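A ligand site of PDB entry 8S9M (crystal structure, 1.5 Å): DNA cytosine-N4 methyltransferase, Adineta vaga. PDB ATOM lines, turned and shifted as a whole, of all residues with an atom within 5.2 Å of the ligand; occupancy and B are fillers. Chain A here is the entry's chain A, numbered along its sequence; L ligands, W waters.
Water W4 lies within hydrogen-bond range of the backbone carbonyl oxygen (O) of Phe 203 (2.7 Å), the side-chain carboxylate (OD2) of Asp 201 (2.8 Å), a nitrogen (N1) of the ligand (2.8 Å) and the backbone NH (N) of Ser 30 (2.9 Å). Water W3 lies within hydrogen-bond range of N of Thr 52 (2.8 Å), O5 of the ligand (2.8 Å) and N of Tyr 53 (3.5 Å). Water W5 lies within hydrogen-bond range of OG of Ser 30 (2.6 Å), O of Pro 31 (2.7 Å) and N2 of the ligand (2.8 Å). Water W1 lies within hydrogen-bond range of O of Ala 178 (2.8 Å), N1 of the ligand (2.9 Å) and OG of Ser 30 (3.5 Å).
An oxygen (O5) of the ligand is in hydrogen-bond range of the side-chain carboxylate (OD1) of Asp 224 (2.7 Å). N of Ser 206 sits at hydrogen-bond distance from O2 of the ligand, at 2.8 Å. The side-chain hydroxyl (OG) of Ser 206 lies within hydrogen-bond range of an oxygen (O2) of the ligand (2.7 Å). An oxygen (O1) of the ligand sits at hydrogen-bond distance from the side-chain hydroxyl of Thr 208 (2.7 Å). N of Ser 12 lies within hydrogen-bond range of N6 of the ligand. N6 of the ligand lies within hydrogen-bond range of OG of Ser 12, 3.3 Å away. N5 of the ligand lies within hydrogen-bond range of OD1 of Asp 11 (2.9 Å). NE2 of His 176 lies within hydrogen-bond range of O4 of the ligand (3.0 Å). OH of Tyr 50 is in hydrogen-bond range of N2 of the ligand (3.0 Å). N of Phe 180 is in hydrogen-bond range of O1 of the ligand, at 3.0 Å. A nitrogen (N2) of the ligand sits at hydrogen-bond distance from the backbone carbonyl oxygen (O) of Ala 178, 3.1 Å away.
The backbone NH (N) of Gly 205 sits at hydrogen-bond distance from the side-chain carboxylate (OD2) of Asp 224. OD1 of Asp 224 is in hydrogen-bond range of N of Ser 226 (3.2 Å). OG1 of Thr 208 is in hydrogen-bond range of OG of Ser 206. The side-chain hydroxyl of Ser 206 is in hydrogen-bond range of the side-chain amide nitrogen of Asn 174 (3.0 Å). OG1 of Thr 208 lies close to O of Phe 180 (3.4 Å). The backbone NH of Ala 178 sits at hydrogen-bond distance from a ring nitrogen (ND1) of His 176 (3.0 Å). N of Tyr 229 is in hydrogen-bond range of OG of Ser 226 (3.0 Å). The backbone NH (N) of Ala 204 is in hydrogen-bond range of the backbone carbonyl oxygen (O) of Phe 223, at 2.8 Å.
Residues that only touch the ligand: Phe 203 (3.4 Å), Tyr 229 (3.4 Å), Gly 205 (3.4 Å), Pro 179 (3.4 Å), Ser 30 (3.5 Å), Ile 225 (3.5 Å), Pro 32 (3.6 Å), Ala 204 (3.7 Å), Trp 65 (3.7 Å), Tyr 53 (3.8 Å), Pro 202 (3.8 Å) and Leu 10 (3.9 Å). Of the 28 residues printed, 21 come within 4 Å of the ligand. The nearest printed residue that does not touch the ligand is Gly 207 (4.2 Å).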
ATOM      1  N   LEU A  10       2.207  22.576  19.479  1.00  0.00           N
ATOM      2  CA  LEU A  10       1.175  23.467  18.952  1.00  0.00           C
ATOM      3  C   LEU A  10       0.433  22.743  17.839  1.00  0.00           C
ATOM      4  O   LEU A  10       1.023  21.962  17.088  1.00  0.00           O
ATOM      5  CB  LEU A  10       1.820  24.737  18.382  1.00  0.00           C
ATOM      6  CG  LEU A  10       0.890  25.868  17.941  1.00  0.00           C
ATOM      7  CD1 LEU A  10       0.054  26.353  19.121  1.00  0.00           C
ATOM      8  CD2 LEU A  10       1.687  27.021  17.349  1.00  0.00           C
ATOM      9  N   ASP A  11      -0.861  23.023  17.745  1.00  0.00           N
ATOM     10  CA  ASP A  11      -1.666  22.539  16.628  1.00  0.00           C
ATOM     11  C   ASP A  11      -1.069  22.996  15.299  1.00  0.00           C
ATOM     12  O   ASP A  11      -0.583  24.130  15.163  1.00  0.00           O
ATOM     13  CB  ASP A  11      -3.087  23.065  16.771  1.00  0.00           C
ATOM     14  CG  ASP A  11      -3.926  22.813  15.537  1.00  0.00           C
ATOM     15  OD1 ASP A  11      -4.357  21.668  15.341  1.00  0.00           O
ATOM     16  OD2 ASP A  11      -4.157  23.762  14.758  1.00  0.00           O
ATOM     17  N   SER A  12      -1.143  22.118  14.300  1.00  0.00           N
ATOM     18  CA  SER A  12      -0.457  22.345  13.030  1.00  0.00           C
ATOM     19  C   SER A  12      -1.009  23.576  12.304  1.00  0.00           C
ATOM     20  O   SER A  12      -0.246  24.396  11.781  1.00  0.00           O
ATOM     21  CB  SER A  12      -0.545  21.099  12.149  1.00  0.00           C
ATOM     22  OG  SER A  12      -1.893  20.692  11.998  1.00  0.00           O
ATOM     23  N   SER A  30       4.394  14.219   6.926  1.00  0.00           N
ATOM     24  CA  SER A  30       3.455  13.127   6.795  1.00  0.00           C
ATOM     25  C   SER A  30       2.385  13.272   7.879  1.00  0.00           C
ATOM     26  O   SER A  30       2.678  13.098   9.065  1.00  0.00           O
ATOM     27  CB  SER A  30       4.175  11.787   6.936  1.00  0.00           C
ATOM     28  OG  SER A  30       3.260  10.710   6.794  1.00  0.00           O
ATOM     29  N   PRO A  31       1.152  13.605   7.504  1.00  0.00           N
ATOM     30  CA  PRO A  31       0.100  13.800   8.510  1.00  0.00           C
ATOM     31  C   PRO A  31      -0.392  12.481   9.045  1.00  0.00           C
ATOM     32  O   PRO A  31      -0.096  11.413   8.474  1.00  0.00           O
ATOM     33  CB  PRO A  31      -1.006  14.483   7.677  1.00  0.00           C
ATOM     34  CG  PRO A  31      -0.877  13.798   6.338  1.00  0.00           C
ATOM     35  CD  PRO A  31       0.630  13.696   6.133  1.00  0.00           C
ATOM     36  N   PRO A  32      -1.165  12.474  10.137  1.00  0.00           N
ATOM     37  CA  PRO A  32      -1.913  11.256  10.467  1.00  0.00           C
ATOM     38  C   PRO A  32      -2.771  10.879   9.278  1.00  0.00           C
ATOM     39  O   PRO A  32      -3.275  11.743   8.549  1.00  0.00           O
ATOM     40  CB  PRO A  32      -2.764  11.688  11.671  1.00  0.00           C
ATOM     41  CG  PRO A  32      -2.855  13.171  11.566  1.00  0.00           C
ATOM     42  CD  PRO A  32      -1.551  13.621  10.974  1.00  0.00           C
ATOM     43  N   TYR A  50      -1.600   7.387  18.513  1.00  0.00           N
ATOM     44  CA  TYR A  50      -0.628   8.398  18.878  1.00  0.00           C
ATOM     45  C   TYR A  50      -0.799   8.795  20.340  1.00  0.00           C
ATOM     46  O   TYR A  50      -1.838   8.551  20.968  1.00  0.00           O
ATOM     47  CB  TYR A  50      -0.789   9.622  17.992  1.00  0.00           C
ATOM     48  CG  TYR A  50      -0.527   9.386  16.525  1.00  0.00           C
ATOM     49  CD1 TYR A  50       0.762   9.121  16.073  1.00  0.00           C
ATOM     50  CD2 TYR A  50      -1.548   9.450  15.597  1.00  0.00           C
ATOM     51  CE1 TYR A  50       1.007   8.927  14.731  1.00  0.00           C
ATOM     52  CE2 TYR A  50      -1.317   9.254  14.251  1.00  0.00           C
ATOM     53  CZ  TYR A  50      -0.023   8.999  13.825  1.00  0.00           C
ATOM     54  OH  TYR A  50       0.230   8.800  12.484  1.00  0.00           O
ATOM     55  N   THR A  52      -1.340  11.607  21.901  1.00  0.00           N
ATOM     56  CA  THR A  52      -2.455  12.482  22.240  1.00  0.00           C
ATOM     57  C   THR A  52      -3.454  12.621  21.092  1.00  0.00           C
ATOM     58  O   THR A  52      -4.204  13.600  21.046  1.00  0.00           O
ATOM     59  CB  THR A  52      -1.965  13.877  22.673  1.00  0.00           C
ATOM     60  OG1 THR A  52      -1.300  14.527  21.579  1.00  0.00           O
ATOM     61  CG2 THR A  52      -0.999  13.764  23.840  1.00  0.00           C
ATOM     62  N   TYR A  53      -3.480  11.662  20.169  1.00  0.00           N
ATOM     63  CA  TYR A  53      -4.380  11.769  19.030  1.00  0.00           C
ATOM     64  C   TYR A  53      -4.872  10.390  18.622  1.00  0.00           C
ATOM     65  O   TYR A  53      -4.056   9.487  18.385  1.00  0.00           O
ATOM     66  CB  TYR A  53      -3.691  12.458  17.846  1.00  0.00           C
ATOM     67  CG  TYR A  53      -4.617  12.698  16.682  1.00  0.00           C
ATOM     68  CD1 TYR A  53      -5.773  13.461  16.849  1.00  0.00           C
ATOM     69  CD2 TYR A  53      -4.344  12.157  15.435  1.00  0.00           C
ATOM     70  CE1 TYR A  53      -6.629  13.672  15.783  1.00  0.00           C
ATOM     71  CE2 TYR A  53      -5.184  12.388  14.357  1.00  0.00           C
ATOM     72  CZ  TYR A  53      -6.329  13.135  14.544  1.00  0.00           C
ATOM     73  OH  TYR A  53      -7.180  13.354  13.481  1.00  0.00           O
ATOM     74  N   TRP A  65      -9.775  19.311   6.515  1.00  0.00           N
ATOM     75  CA  TRP A  65      -8.653  19.741   7.352  1.00  0.00           C
ATOM     76  C   TRP A  65      -7.344  19.659   6.591  1.00  0.00           C
ATOM     77  O   TRP A  65      -6.546  20.607   6.598  1.00  0.00           O
ATOM     78  CB  TRP A  65      -8.635  18.859   8.595  1.00  0.00           C
ATOM     79  CG  TRP A  65      -7.473  19.043   9.514  1.00  0.00           C
ATOM     80  CD1 TRP A  65      -6.969  20.222   9.998  1.00  0.00           C
ATOM     81  CD2 TRP A  65      -6.711  18.008  10.128  1.00  0.00           C
ATOM     82  NE1 TRP A  65      -5.925  19.974  10.848  1.00  0.00           N
ATOM     83  CE2 TRP A  65      -5.745  18.614  10.949  1.00  0.00           C
ATOM     84  CE3 TRP A  65      -6.754  16.608  10.057  1.00  0.00           C
ATOM     85  CZ2 TRP A  65      -4.823  17.889  11.696  1.00  0.00           C
ATOM     86  CZ3 TRP A  65      -5.835  15.877  10.791  1.00  0.00           C
ATOM     87  CH2 TRP A  65      -4.878  16.522  11.598  1.00  0.00           C
ATOM     88  N   ASN A 174      12.832   3.360  15.433  1.00  0.00           N
ATOM     89  CA  ASN A 174      12.215   4.577  15.955  1.00  0.00           C
ATOM     90  C   ASN A 174      10.993   4.183  16.779  1.00  0.00           C
ATOM     91  O   ASN A 174      10.117   3.449  16.293  1.00  0.00           O
ATOM     92  CB  ASN A 174      11.815   5.447  14.761  1.00  0.00           C
ATOM     93  CG  ASN A 174      11.374   6.843  15.146  1.00  0.00           C
ATOM     94  OD1 ASN A 174      10.672   7.045  16.134  1.00  0.00           O
ATOM     95  ND2 ASN A 174      11.766   7.816  14.335  1.00  0.00           N
ATOM     96  N   HIS A 176       8.538   6.043  17.821  1.00  0.00           N
ATOM     97  CA  HIS A 176       7.296   6.689  17.425  1.00  0.00           C
ATOM     98  C   HIS A 176       6.444   5.693  16.635  1.00  0.00           C
ATOM     99  O   HIS A 176       6.992   4.872  15.893  1.00  0.00           O
ATOM    100  CB  HIS A 176       7.633   7.887  16.543  1.00  0.00           C
ATOM    101  CG  HIS A 176       6.449   8.721  16.161  1.00  0.00           C
ATOM    102  ND1 HIS A 176       5.596   8.369  15.132  1.00  0.00           N
ATOM    103  CD2 HIS A 176       5.967   9.883  16.663  1.00  0.00           C
ATOM    104  CE1 HIS A 176       4.643   9.282  15.021  1.00  0.00           C
ATOM    105  NE2 HIS A 176       4.858  10.209  15.934  1.00  0.00           N
ATOM    106  N   ALA A 178       4.544   5.805  13.975  1.00  0.00           N
ATOM    107  CA  ALA A 178       4.428   5.869  12.518  1.00  0.00           C
ATOM    108  C   ALA A 178       5.352   6.946  11.962  1.00  0.00           C
ATOM    109  O   ALA A 178       4.911   7.958  11.432  1.00  0.00           O
ATOM    110  CB  ALA A 178       2.988   6.131  12.097  1.00  0.00           C
ATOM    111  N   PRO A 179       6.677   6.723  12.027  1.00  0.00           N
ATOM    112  CA  PRO A 179       7.629   7.726  11.534  1.00  0.00           C
ATOM    113  C   PRO A 179       8.060   7.437  10.100  1.00  0.00           C
ATOM    114  O   PRO A 179       7.725   6.367   9.555  1.00  0.00           O
ATOM    115  CB  PRO A 179       8.816   7.533  12.473  1.00  0.00           C
ATOM    116  CG  PRO A 179       8.834   6.008  12.664  1.00  0.00           C
ATOM    117  CD  PRO A 179       7.375   5.558  12.598  1.00  0.00           C
ATOM    118  N   PHE A 180       8.803   8.339   9.487  1.00  0.00           N
ATOM    119  CA  PHE A 180       9.508   8.027   8.264  1.00  0.00           C
ATOM    120  C   PHE A 180      11.011   8.107   8.476  1.00  0.00           C
ATOM    121  O   PHE A 180      11.475   8.702   9.463  1.00  0.00           O
ATOM    122  CB  PHE A 180       9.026   8.830   7.029  1.00  0.00           C
ATOM    123  CG  PHE A 180       9.005  10.342   7.199  1.00  0.00           C
ATOM    124  CD1 PHE A 180      10.128  11.048   7.586  1.00  0.00           C
ATOM    125  CD2 PHE A 180       7.864  11.049   6.859  1.00  0.00           C
ATOM    126  CE1 PHE A 180      10.096  12.432   7.685  1.00  0.00           C
ATOM    127  CE2 PHE A 180       7.817  12.430   6.963  1.00  0.00           C
ATOM    128  CZ  PHE A 180       8.940  13.122   7.379  1.00  0.00           C
ATOM    129  N   ASP A 201       8.291  21.126   9.278  1.00  0.00           N
ATOM    130  CA  ASP A 201       7.439  19.940   9.360  1.00  0.00           C
ATOM    131  C   ASP A 201       6.300  20.231  10.314  1.00  0.00           C
ATOM    132  O   ASP A 201       6.504  20.265  11.544  1.00  0.00           O
ATOM    133  CB  ASP A 201       8.200  18.673   9.781  1.00  0.00           C
ATOM    134  CG  ASP A 201       7.347  17.408   9.647  1.00  0.00           C
ATOM    135  OD1 ASP A 201       6.097  17.517   9.636  1.00  0.00           O
ATOM    136  OD2 ASP A 201       7.922  16.300   9.531  1.00  0.00           O
ATOM    137  N   PRO A 202       5.075  20.439   9.810  1.00  0.00           N
ATOM    138  CA  PRO A 202       3.963  20.780  10.700  1.00  0.00           C
ATOM    139  C   PRO A 202       3.306  19.592  11.386  1.00  0.00           C
ATOM    140  O   PRO A 202       2.348  19.787  12.149  1.00  0.00           O
ATOM    141  CB  PRO A 202       2.975  21.476   9.754  1.00  0.00           C
ATOM    142  CG  PRO A 202       3.211  20.790   8.455  1.00  0.00           C
ATOM    143  CD  PRO A 202       4.707  20.551   8.392  1.00  0.00           C
ATOM    144  N   PHE A 203       3.808  18.368  11.153  1.00  0.00           N
ATOM    145  CA  PHE A 203       3.410  17.169  11.877  1.00  0.00           C
ATOM    146  C   PHE A 203       4.691  16.426  12.312  1.00  0.00           C
ATOM    147  O   PHE A 203       4.971  15.317  11.876  1.00  0.00           O
ATOM    148  CB  PHE A 203       2.543  16.247  11.007  1.00  0.00           C
ATOM    149  CG  PHE A 203       1.196  16.821  10.668  1.00  0.00           C
ATOM    150  CD1 PHE A 203       0.179  16.868  11.610  1.00  0.00           C
ATOM    151  CD2 PHE A 203       0.937  17.309   9.397  1.00  0.00           C
ATOM    152  CE1 PHE A 203      -1.071  17.391  11.295  1.00  0.00           C
ATOM    153  CE2 PHE A 203      -0.295  17.840   9.068  1.00  0.00           C
ATOM    154  CZ  PHE A 203      -1.306  17.878  10.019  1.00  0.00           C
ATOM    155  N   ALA A 204       5.469  17.069  13.186  1.00  0.00           N
ATOM    156  CA  ALA A 204       6.887  16.723  13.297  1.00  0.00           C
ATOM    157  C   ALA A 204       7.121  15.347  13.935  1.00  0.00           C
ATOM    158  O   ALA A 204       8.143  14.709  13.637  1.00  0.00           O
ATOM    159  CB  ALA A 204       7.639  17.816  14.053  1.00  0.00           C
ATOM    160  N   GLY A 205       6.218  14.869  14.784  1.00  0.00           N
ATOM    161  CA  GLY A 205       6.381  13.542  15.362  1.00  0.00           C
ATOM    162  C   GLY A 205       7.698  13.390  16.112  1.00  0.00           C
ATOM    163  O   GLY A 205       8.041  14.182  16.991  1.00  0.00           O
ATOM    164  N   SER A 206       8.440  12.349  15.751  1.00  0.00           N
ATOM    165  CA  SER A 206       9.754  12.104  16.345  1.00  0.00           C
ATOM    166  C   SER A 206      10.813  13.106  15.892  1.00  0.00           C
ATOM    167  O   SER A 206      11.967  12.997  16.318  1.00  0.00           O
ATOM    168  CB  SER A 206      10.222  10.671  16.054  1.00  0.00           C
ATOM    169  OG  SER A 206      10.542  10.493  14.685  1.00  0.00           O
ATOM    170  N   GLY A 207      10.462  14.049  15.024  1.00  0.00           N
ATOM    171  CA  GLY A 207      11.380  15.103  14.632  1.00  0.00           C
ATOM    172  C   GLY A 207      12.302  14.744  13.501  1.00  0.00           C
ATOM    173  O   GLY A 207      13.291  15.451  13.280  1.00  0.00           O
ATOM    174  N   THR A 208      12.002  13.682  12.752  1.00  0.00           N
ATOM    175  CA  THR A 208      12.862  13.208  11.679  1.00  0.00           C
ATOM    176  C   THR A 208      13.269  14.325  10.729  1.00  0.00           C
ATOM    177  O   THR A 208      14.451  14.458  10.380  1.00  0.00           O
ATOM    178  CB  THR A 208      12.126  12.120  10.918  1.00  0.00           C
ATOM    179  OG1 THR A 208      11.700  11.113  11.850  1.00  0.00           O
ATOM    180  CG2 THR A 208      13.031  11.507   9.883  1.00  0.00           C
ATOM    181  N   PHE A 223       6.049  21.471  14.304  1.00  0.00           N
ATOM    182  CA  PHE A 223       4.906  21.509  15.197  1.00  0.00           C
ATOM    183  C   PHE A 223       4.398  20.097  15.432  1.00  0.00           C
ATOM    184  O   PHE A 223       4.387  19.282  14.512  1.00  0.00           O
ATOM    185  CB  PHE A 223       3.740  22.305  14.595  1.00  0.00           C
ATOM    186  CG  PHE A 223       4.121  23.643  14.066  1.00  0.00           C
ATOM    187  CD1 PHE A 223       4.739  24.587  14.861  1.00  0.00           C
ATOM    188  CD2 PHE A 223       3.825  23.971  12.750  1.00  0.00           C
ATOM    189  CE1 PHE A 223       5.077  25.831  14.347  1.00  0.00           C
ATOM    190  CE2 PHE A 223       4.157  25.207  12.233  1.00  0.00           C
ATOM    191  CZ  PHE A 223       4.792  26.139  13.029  1.00  0.00           C
ATOM    192  N   ASP A 224       3.958  19.830  16.654  1.00  0.00           N
ATOM    193  CA  ASP A 224       3.205  18.620  16.974  1.00  0.00           C
ATOM    194  C   ASP A 224       2.443  18.908  18.248  1.00  0.00           C
ATOM    195  O   ASP A 224       2.764  19.844  18.989  1.00  0.00           O
ATOM    196  CB  ASP A 224       4.150  17.408  17.127  1.00  0.00           C
ATOM    197  CG  ASP A 224       3.424  16.058  16.963  1.00  0.00           C
ATOM    198  OD1 ASP A 224       2.510  15.750  17.770  1.00  0.00           O
ATOM    199  OD2 ASP A 224       3.790  15.288  16.043  1.00  0.00           O
ATOM    200  N   ILE A 225       1.391  18.116  18.493  1.00  0.00           N
ATOM    201  CA  ILE A 225       0.568  18.328  19.686  1.00  0.00           C
ATOM    202  C   ILE A 225       1.047  17.553  20.896  1.00  0.00           C
ATOM    203  O   ILE A 225       0.447  17.684  21.969  1.00  0.00           O
ATOM    204  CB  ILE A 225      -0.935  18.102  19.401  1.00  0.00           C
ATOM    205  CG1 ILE A 225      -1.152  16.723  18.792  1.00  0.00           C
ATOM    206  CG2 ILE A 225      -1.463  19.188  18.480  1.00  0.00           C
ATOM    207  CD1 ILE A 225      -2.610  16.351  18.641  1.00  0.00           C
ATOM    208  N   SER A 226       2.104  16.759  20.769  1.00  0.00           N
ATOM    209  CA  SER A 226       2.553  15.874  21.843  1.00  0.00           C
ATOM    210  C   SER A 226       3.853  16.387  22.441  1.00  0.00           C
ATOM    211  O   SER A 226       4.872  16.477  21.754  1.00  0.00           O
ATOM    212  CB  SER A 226       2.759  14.459  21.310  1.00  0.00           C
ATOM    213  OG  SER A 226       3.508  13.685  22.242  1.00  0.00           O
ATOM    214  N   TYR A 229       6.485  13.589  22.176  1.00  0.00           N
ATOM    215  CA  TYR A 229       7.227  13.535  20.928  1.00  0.00           C
ATOM    216  C   TYR A 229       8.243  14.673  20.825  1.00  0.00           C
ATOM    217  O   TYR A 229       9.308  14.493  20.236  1.00  0.00           O
ATOM    218  CB  TYR A 229       6.276  13.546  19.736  1.00  0.00           C
ATOM    219  CG  TYR A 229       5.361  12.323  19.683  1.00  0.00           C
ATOM    220  CD1 TYR A 229       5.660  11.167  20.391  1.00  0.00           C
ATOM    221  CD2 TYR A 229       4.198  12.347  18.930  1.00  0.00           C
ATOM    222  CE1 TYR A 229       4.820  10.051  20.336  1.00  0.00           C
ATOM    223  CE2 TYR A 229       3.361  11.249  18.859  1.00  0.00           C
ATOM    224  CZ  TYR A 229       3.668  10.104  19.561  1.00  0.00           C
ATOM    225  OH  TYR A 229       2.808   9.028  19.501  1.00  0.00           O
HETATM  226  N1  LIG L   1       6.922  11.868  10.094  1.00  0.00           N
HETATM  227  C1  LIG L   1       6.947  11.870  11.566  1.00  0.00           C
HETATM  228  C2  LIG L   1       8.198  11.142  12.039  1.00  0.00           C
HETATM  229  O1  LIG L   1       9.069  10.788  11.271  1.00  0.00           O
HETATM  230  O2  LIG L   1       8.238  10.970  13.337  1.00  0.00           O
HETATM  231  C3  LIG L   1       5.688  11.265  12.202  1.00  0.00           C
HETATM  232  C4  LIG L   1       4.389  12.013  11.893  1.00  0.00           C
HETATM  233  C5  LIG L   1       3.134  11.334  12.435  1.00  0.00           C
HETATM  234  N2  LIG L   1       2.788  10.151  11.650  1.00  0.00           N
HETATM  235  C6  LIG L   1       1.927  12.275  12.518  1.00  0.00           C
HETATM  236  C7  LIG L   1       1.967  13.214  13.708  1.00  0.00           C
HETATM  237  O3  LIG L   1       0.867  14.135  13.654  1.00  0.00           O
HETATM  238  C8  LIG L   1       1.901  12.542  15.094  1.00  0.00           C
HETATM  239  O4  LIG L   1       3.149  12.661  15.750  1.00  0.00           O
HETATM  240  C9  LIG L   1       0.774  13.308  15.818  1.00  0.00           C
HETATM  241  O5  LIG L   1       1.057  13.588  17.183  1.00  0.00           O
HETATM  242  C10 LIG L   1       0.708  14.586  14.985  1.00  0.00           C
HETATM  243  N3  LIG L   1      -0.525  15.352  15.065  1.00  0.00           N
HETATM  244  C11 LIG L   1      -1.827  14.923  15.061  1.00  0.00           C
HETATM  245  N4  LIG L   1      -2.714  15.888  15.048  1.00  0.00           N
HETATM  246  C12 LIG L   1      -1.941  17.041  15.041  1.00  0.00           C
HETATM  247  C13 LIG L   1      -2.272  18.404  15.006  1.00  0.00           C
HETATM  248  N5  LIG L   1      -3.523  18.864  15.050  1.00  0.00           N
HETATM  249  N6  LIG L   1      -1.262  19.299  14.962  1.00  0.00           N
HETATM  250  C14 LIG L   1       0.000  18.844  14.977  1.00  0.00           C
HETATM  251  N7  LIG L   1       0.441  17.587  15.039  1.00  0.00           N
HETATM  252  C15 LIG L   1      -0.594  16.723  15.053  1.00  0.00           C
HETATM  253  O   HOH W   1       5.461   9.556   9.204  1.00  0.00           O
HETATM  254  O   HOH W   2      -5.495  16.795  15.418  1.00  0.00           O
HETATM  255  O   HOH W   3      -0.249  12.722  19.541  1.00  0.00           O
HETATM  256  O   HOH W   4       5.885  14.416   9.460  1.00  0.00           O
HETATM  257  O   HOH W   5       2.063   9.882   8.915  1.00  0.00           O
